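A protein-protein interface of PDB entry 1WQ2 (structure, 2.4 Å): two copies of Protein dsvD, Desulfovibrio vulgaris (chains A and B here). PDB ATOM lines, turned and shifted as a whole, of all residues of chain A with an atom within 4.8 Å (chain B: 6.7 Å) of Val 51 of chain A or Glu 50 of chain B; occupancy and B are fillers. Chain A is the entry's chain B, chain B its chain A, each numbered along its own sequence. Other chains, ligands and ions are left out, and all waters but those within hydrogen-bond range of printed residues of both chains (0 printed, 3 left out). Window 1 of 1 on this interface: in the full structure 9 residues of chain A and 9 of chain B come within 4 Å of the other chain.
The side-chain amide oxygen (OE1) of Gln 6 of chain A lies close to the side-chain carboxylate (OE2) of Glu 50 of chain B (2.7 Å).
Asp 49 of chain A touches Val 51 of chain B, and with the chains exchanged Val 51 of chain A touches Asp 49 of chain B. Val 51 of chain A touches Glu 50 of chain B, but with the chains exchanged Glu 50 of chain A does not touch Val 51 of chain B (4.1 Å). Leu 65 of chain A touches Lys 66 of chain B, and with the chains exchanged Lys 66 of chain A touches Leu 65 of chain B. Positions printed for both chains: 46, 49, 50, 51, 52, 53, 65 and 66. Of the 8 pairs that touch across the chains among the printed residues, 4 have their exchanged pair printed and touching as well.
Of the printed residues of chain B, Gln 6 of chain A touches Glu 50. Of chain B, only Asp 49 (3.8 Å) and Glu 50 (3.9 Å) come within 4 Å of Val 51 of chain A. Printed residues of chain B within 4 Å of Leu 65 of chain A: Lys 66. Of the printed residues of chain A, Asp 49 of chain B touches Val 51 (3.8 Å). Glu 50 of chain B touches just these residues of chain A: Gln 6 (2.7 Å), Val 9 (3.6 Å) and Val 51 (3.9 Å). The nearest printed residue of chain B that does not touch Leu 65 of chain A is Gly 67 of chain B (4.004 Å).
Of the 12 printed residues of chain B, 5 touch a printed residue of chain A. Printed residues of chain B that touch a printed residue of chain A: Asp 49, Glu 50, Val 51, Leu 65 and Lys 66. Of the 12 printed residues of chain A, 6 touch a printed residue of chain B. Among the printed residues, 8 pairs touch across the chains. Among the printed residues, no Asp or Glu carboxylate lies within 4 Å of a Lys or Arg side-chain nitrogen of the other chain.
Among the printed residues, pairs that only touch across the chains: Val 9 of chain A with Glu 50 of chain B (3.6 Å), Val 9 of chain A with Lys 66 of chain B (3.8 Å), Asp 49 of chain A with Val 51 of chain B (3.6 Å), Val 51 of chain A with Asp 49 of chain B (3.8 Å), Val 51 of chain A with Glu 50 of chain B (3.9 Å), Leu 65 of chain A with Lys 66 of chain B (3.6 Å) and Lys 66 of chain A with Leu 65 of chain B (3.8 Å).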
ATOM      1  N   MET A   1      -4.257  15.917 -21.230  1.00  0.00           N
ATOM      2  CA  MET A   1      -3.586  16.538 -20.085  1.00  0.00           C
ATOM      3  C   MET A   1      -3.922  18.024 -20.007  1.00  0.00           C
ATOM      4  O   MET A   1      -4.637  18.539 -20.869  1.00  0.00           O
ATOM      5  N   GLN A   6       0.213  20.033 -22.613  1.00  0.00           N
ATOM      6  CA  GLN A   6      -0.146  19.726 -23.985  1.00  0.00           C
ATOM      7  C   GLN A   6       0.610  20.661 -24.924  1.00  0.00           C
ATOM      8  O   GLN A   6       0.941  20.285 -26.052  1.00  0.00           O
ATOM      9  CB  GLN A   6      -1.658  19.887 -24.180  1.00  0.00           C
ATOM     10  CG  GLN A   6      -2.158  19.338 -25.508  1.00  0.00           C
ATOM     11  CD  GLN A   6      -1.841  17.865 -25.678  1.00  0.00           C
ATOM     12  OE1 GLN A   6      -2.334  17.020 -24.934  1.00  0.00           O
ATOM     13  NE2 GLN A   6      -1.005  17.553 -26.658  1.00  0.00           N
ATOM     14  N   VAL A   9       3.938  19.161 -25.472  1.00  0.00           N
ATOM     15  CA  VAL A   9       3.845  17.982 -26.336  1.00  0.00           C
ATOM     16  C   VAL A   9       3.646  18.319 -27.812  1.00  0.00           C
ATOM     17  O   VAL A   9       4.244  17.681 -28.671  1.00  0.00           O
ATOM     18  CB  VAL A   9       2.719  17.025 -25.873  1.00  0.00           C
ATOM     19  CG1 VAL A   9       2.627  15.826 -26.812  1.00  0.00           C
ATOM     20  CG2 VAL A   9       2.986  16.542 -24.456  1.00  0.00           C
ATOM     21  N   LEU A  46       6.159  15.583 -16.732  1.00  0.00           N
ATOM     22  CA  LEU A  46       6.079  14.887 -18.010  1.00  0.00           C
ATOM     23  C   LEU A  46       7.136  13.787 -18.064  1.00  0.00           C
ATOM     24  O   LEU A  46       6.924  12.753 -18.690  1.00  0.00           O
ATOM     25  CB  LEU A  46       6.249  15.870 -19.175  1.00  0.00           C
ATOM     26  CG  LEU A  46       5.013  16.739 -19.444  1.00  0.00           C
ATOM     27  CD1 LEU A  46       5.309  17.732 -20.554  1.00  0.00           C
ATOM     28  CD2 LEU A  46       3.844  15.852 -19.842  1.00  0.00           C
ATOM     29  N   ASP A  49       5.842  10.836 -15.968  1.00  0.00           N
ATOM     30  CA  ASP A  49       4.820  10.056 -16.647  1.00  0.00           C
ATOM     31  C   ASP A  49       5.361   9.385 -17.907  1.00  0.00           C
ATOM     32  O   ASP A  49       4.620   8.739 -18.648  1.00  0.00           O
ATOM     33  CB  ASP A  49       3.603  10.938 -16.948  1.00  0.00           C
ATOM     34  CG  ASP A  49       2.809  11.278 -15.688  1.00  0.00           C
ATOM     35  OD1 ASP A  49       2.530  12.472 -15.456  1.00  0.00           O
ATOM     36  OD2 ASP A  49       2.473  10.349 -14.921  1.00  0.00           O
ATOM     37  N   GLU A  50       6.668   9.533 -18.121  1.00  0.00           N
ATOM     38  CA  GLU A  50       7.397   8.938 -19.239  1.00  0.00           C
ATOM     39  C   GLU A  50       7.050   9.418 -20.638  1.00  0.00           C
ATOM     40  O   GLU A  50       7.310   8.735 -21.627  1.00  0.00           O
ATOM     41  CB  GLU A  50       7.329   7.419 -19.152  1.00  0.00           C
ATOM     42  CG  GLU A  50       8.251   6.883 -18.080  1.00  0.00           C
ATOM     43  CD  GLU A  50       8.291   5.378 -18.051  1.00  0.00           C
ATOM     44  OE1 GLU A  50       7.969   4.810 -16.990  1.00  0.00           O
ATOM     45  OE2 GLU A  50       8.652   4.769 -19.082  1.00  0.00           O
ATOM     46  N   VAL A  51       6.485  10.613 -20.709  1.00  0.00           N
ATOM     47  CA  VAL A  51       6.153  11.243 -21.977  1.00  0.00           C
ATOM     48  C   VAL A  51       7.463  11.799 -22.537  1.00  0.00           C
ATOM     49  O   VAL A  51       7.727  11.700 -23.734  1.00  0.00           O
ATOM     50  CB  VAL A  51       5.153  12.401 -21.779  1.00  0.00           C
ATOM     51  CG1 VAL A  51       4.884  13.107 -23.107  1.00  0.00           C
ATOM     52  CG2 VAL A  51       3.851  11.862 -21.201  1.00  0.00           C
ATOM     53  N   LEU A  52       8.295  12.343 -21.645  1.00  0.00           N
ATOM     54  CA  LEU A  52       9.587  12.926 -22.015  1.00  0.00           C
ATOM     55  C   LEU A  52      10.761  12.186 -21.378  1.00  0.00           C
ATOM     56  O   LEU A  52      10.616  11.563 -20.328  1.00  0.00           O
ATOM     57  CB  LEU A  52       9.666  14.390 -21.559  1.00  0.00           C
ATOM     58  CG  LEU A  52       8.588  15.350 -22.058  1.00  0.00           C
ATOM     59  CD1 LEU A  52       8.920  16.752 -21.568  1.00  0.00           C
ATOM     60  CD2 LEU A  52       8.495  15.319 -23.576  1.00  0.00           C
ATOM     61  N   GLU A  53      11.917  12.267 -22.033  1.00  0.00           N
ATOM     62  CA  GLU A  53      13.149  11.673 -21.538  1.00  0.00           C
ATOM     63  C   GLU A  53      13.986  12.850 -21.011  1.00  0.00           C
ATOM     64  O   GLU A  53      13.947  13.944 -21.576  1.00  0.00           O
ATOM     65  CB  GLU A  53      13.878  10.887 -22.650  1.00  0.00           C
ATOM     66  CG  GLU A  53      14.067  11.635 -23.976  1.00  0.00           C
ATOM     67  CD  GLU A  53      14.548  10.743 -25.132  1.00  0.00           C
ATOM     68  OE1 GLU A  53      14.769  11.285 -26.239  1.00  0.00           O
ATOM     69  OE2 GLU A  53      14.708   9.514 -24.950  1.00  0.00           O
ATOM     70  N   GLY A  64      13.282  15.748 -24.221  1.00  0.00           N
ATOM     71  CA  GLY A  64      12.806  15.362 -25.536  1.00  0.00           C
ATOM     72  C   GLY A  64      11.811  14.225 -25.457  1.00  0.00           C
ATOM     73  O   GLY A  64      11.718  13.553 -24.436  1.00  0.00           O
ATOM     74  N   LEU A  65      11.021  14.048 -26.510  1.00  0.00           N
ATOM     75  CA  LEU A  65      10.041  12.968 -26.554  1.00  0.00           C
ATOM     76  C   LEU A  65      10.729  11.630 -26.291  1.00  0.00           C
ATOM     77  O   LEU A  65      11.794  11.354 -26.840  1.00  0.00           O
ATOM     78  CB  LEU A  65       9.334  12.927 -27.918  1.00  0.00           C
ATOM     79  CG  LEU A  65       8.298  14.029 -28.158  1.00  0.00           C
ATOM     80  CD1 LEU A  65       7.757  13.931 -29.578  1.00  0.00           C
ATOM     81  CD2 LEU A  65       7.163  13.886 -27.158  1.00  0.00           C
ATOM     82  N   LYS A  66      10.142  10.840 -25.399  1.00  0.00           N
ATOM     83  CA  LYS A  66      10.659   9.518 -25.046  1.00  0.00           C
ATOM     84  C   LYS A  66      10.862   8.704 -26.330  1.00  0.00           C
ATOM     85  O   LYS A  66       9.933   8.527 -27.120  1.00  0.00           O
ATOM     86  CB  LYS A  66       9.644   8.816 -24.139  1.00  0.00           C
ATOM     87  CG  LYS A  66      10.144   7.560 -23.455  1.00  0.00           C
ATOM     88  CD  LYS A  66      10.886   7.881 -22.176  1.00  0.00           C
ATOM     89  CE  LYS A  66      11.193   6.607 -21.417  1.00  0.00           C
ATOM     90  NZ  LYS A  66      11.928   6.900 -20.163  1.00  0.00           N
ATOM     91  N   ALA B  45      -4.988   3.372 -22.791  1.00  0.00           N
ATOM     92  CA  ALA B  45      -4.690   4.223 -21.638  1.00  0.00           C
ATOM     93  C   ALA B  45      -3.371   4.964 -21.842  1.00  0.00           C
ATOM     94  O   ALA B  45      -3.179   6.058 -21.318  1.00  0.00           O
ATOM     95  CB  ALA B  45      -4.621   3.381 -20.371  1.00  0.00           C
ATOM     96  N   LEU B  46      -2.463   4.353 -22.598  1.00  0.00           N
ATOM     97  CA  LEU B  46      -1.161   4.947 -22.888  1.00  0.00           C
ATOM     98  C   LEU B  46      -1.284   5.980 -24.002  1.00  0.00           C
ATOM     99  O   LEU B  46      -0.500   6.926 -24.066  1.00  0.00           O
ATOM    100  CB  LEU B  46      -0.160   3.858 -23.282  1.00  0.00           C
ATOM    101  CG  LEU B  46       0.434   3.074 -22.110  1.00  0.00           C
ATOM    102  CD1 LEU B  46       1.245   1.916 -22.654  1.00  0.00           C
ATOM    103  CD2 LEU B  46       1.309   3.981 -21.260  1.00  0.00           C
ATOM    104  N   VAL B  47      -2.281   5.804 -24.864  1.00  0.00           N
ATOM    105  CA  VAL B  47      -2.510   6.741 -25.954  1.00  0.00           C
ATOM    106  C   VAL B  47      -3.186   7.977 -25.367  1.00  0.00           C
ATOM    107  O   VAL B  47      -2.899   9.100 -25.779  1.00  0.00           O
ATOM    108  CB  VAL B  47      -3.395   6.125 -27.059  1.00  0.00           C
ATOM    109  CG1 VAL B  47      -3.776   7.197 -28.081  1.00  0.00           C
ATOM    110  CG2 VAL B  47      -2.635   4.997 -27.756  1.00  0.00           C
ATOM    111  N   ASN B  48      -4.062   7.755 -24.383  1.00  0.00           N
ATOM    112  CA  ASN B  48      -4.775   8.831 -23.699  1.00  0.00           C
ATOM    113  C   ASN B  48      -3.763   9.729 -22.988  1.00  0.00           C
ATOM    114  O   ASN B  48      -3.858  10.950 -23.042  1.00  0.00           O
ATOM    115  CB  ASN B  48      -5.731   8.257 -22.636  1.00  0.00           C
ATOM    116  CG  ASN B  48      -6.957   7.586 -23.235  1.00  0.00           C
ATOM    117  OD1 ASN B  48      -7.348   6.494 -22.818  1.00  0.00           O
ATOM    118  ND2 ASN B  48      -7.592   8.250 -24.186  1.00  0.00           N
ATOM    119  N   ASP B  49      -2.782   9.096 -22.345  1.00  0.00           N
ATOM    120  CA  ASP B  49      -1.739   9.783 -21.585  1.00  0.00           C
ATOM    121  C   ASP B  49      -0.658  10.357 -22.483  1.00  0.00           C
ATOM    122  O   ASP B  49       0.227  11.083 -22.023  1.00  0.00           O
ATOM    123  CB  ASP B  49      -1.120   8.823 -20.559  1.00  0.00           C
ATOM    124  CG  ASP B  49      -2.070   8.500 -19.406  1.00  0.00           C
ATOM    125  OD1 ASP B  49      -1.672   7.720 -18.519  1.00  0.00           O
ATOM    126  OD2 ASP B  49      -3.205   9.031 -19.371  1.00  0.00           O
ATOM    127  N   GLU B  50      -0.722   9.991 -23.756  1.00  0.00           N
ATOM    128  CA  GLU B  50       0.206  10.458 -24.785  1.00  0.00           C
ATOM    129  C   GLU B  50       1.637   9.953 -24.668  1.00  0.00           C
ATOM    130  O   GLU B  50       2.592  10.631 -25.047  1.00  0.00           O
ATOM    131  CB  GLU B  50       0.150  11.981 -24.888  1.00  0.00           C
ATOM    132  CG  GLU B  50      -1.178  12.429 -25.479  1.00  0.00           C
ATOM    133  CD  GLU B  50      -1.380  13.918 -25.423  1.00  0.00           C
ATOM    134  OE1 GLU B  50      -0.658  14.636 -26.143  1.00  0.00           O
ATOM    135  OE2 GLU B  50      -2.262  14.370 -24.661  1.00  0.00           O
ATOM    136  N   VAL B  51       1.765   8.756 -24.105  1.00  0.00           N
ATOM    137  CA  VAL B  51       3.042   8.074 -23.994  1.00  0.00           C
ATOM    138  C   VAL B  51       3.198   7.390 -25.358  1.00  0.00           C
ATOM    139  O   VAL B  51       4.285   7.347 -25.930  1.00  0.00           O
ATOM    140  CB  VAL B  51       3.007   7.022 -22.863  1.00  0.00           C
ATOM    141  CG1 VAL B  51       4.306   6.229 -22.839  1.00  0.00           C
ATOM    142  CG2 VAL B  51       2.792   7.712 -21.518  1.00  0.00           C
ATOM    143  N   LEU B  52       2.081   6.883 -25.877  1.00  0.00           N
ATOM    144  CA  LEU B  52       2.026   6.223 -27.175  1.00  0.00           C
ATOM    145  C   LEU B  52       1.127   7.002 -28.136  1.00  0.00           C
ATOM    146  O   LEU B  52       0.413   7.927 -27.734  1.00  0.00           O
ATOM    147  CB  LEU B  52       1.452   4.808 -27.030  1.00  0.00           C
ATOM    148  CG  LEU B  52       2.219   3.818 -26.154  1.00  0.00           C
ATOM    149  CD1 LEU B  52       1.641   2.423 -26.352  1.00  0.00           C
ATOM    150  CD2 LEU B  52       3.692   3.836 -26.502  1.00  0.00           C
ATOM    151  N   GLU B  53       1.217   6.653 -29.418  1.00  0.00           N
ATOM    152  CA  GLU B  53       0.381   7.248 -30.454  1.00  0.00           C
ATOM    153  C   GLU B  53       0.035   6.121 -31.417  1.00  0.00           C
ATOM    154  O   GLU B  53       0.923   5.379 -31.847  1.00  0.00           O
ATOM    155  CB  GLU B  53       1.102   8.385 -31.188  1.00  0.00           C
ATOM    156  CG  GLU B  53       2.362   7.980 -31.945  1.00  0.00           C
ATOM    157  CD  GLU B  53       2.888   9.099 -32.820  1.00  0.00           C
ATOM    158  OE1 GLU B  53       3.268   8.815 -33.968  1.00  0.00           O
ATOM    159  OE2 GLU B  53       2.913  10.259 -32.373  1.00  0.00           O
ATOM    160  N   LEU B  65       5.802   4.942 -29.845  1.00  0.00           N
ATOM    161  CA  LEU B  65       6.073   5.965 -28.844  1.00  0.00           C
ATOM    162  C   LEU B  65       5.707   7.315 -29.439  1.00  0.00           C
ATOM    163  O   LEU B  65       5.949   7.559 -30.620  1.00  0.00           O
ATOM    164  CB  LEU B  65       7.552   5.950 -28.448  1.00  0.00           C
ATOM    165  CG  LEU B  65       7.956   4.803 -27.515  1.00  0.00           C
ATOM    166  CD1 LEU B  65       9.462   4.793 -27.325  1.00  0.00           C
ATOM    167  CD2 LEU B  65       7.274   4.979 -26.163  1.00  0.00           C
ATOM    168  N   LYS B  66       5.103   8.175 -28.624  1.00  0.00           N
ATOM    169  CA  LYS B  66       4.674   9.503 -29.053  1.00  0.00           C
ATOM    170  C   LYS B  66       5.724  10.208 -29.920  1.00  0.00           C
ATOM    171  O   LYS B  66       6.855  10.446 -29.497  1.00  0.00           O
ATOM    172  CB  LYS B  66       4.356  10.354 -27.827  1.00  0.00           C
ATOM    173  CG  LYS B  66       3.721  11.694 -28.143  1.00  0.00           C
ATOM    174  CD  LYS B  66       2.351  11.511 -28.747  1.00  0.00           C
ATOM    175  CE  LYS B  66       1.613  12.825 -28.821  1.00  0.00           C
ATOM    176  NZ  LYS B  66       0.262  12.573 -29.355  1.00  0.00           N
ATOM    177  N   GLY B  67       5.313  10.562 -31.131  1.00  0.00           N
ATOM    178  CA  GLY B  67       6.192  11.220 -32.075  1.00  0.00           C
ATOM    179  C   GLY B  67       6.769  10.272 -33.111  1.00  0.00           C
ATOM    180  O   GLY B  67       7.505  10.710 -33.995  1.00  0.00           O
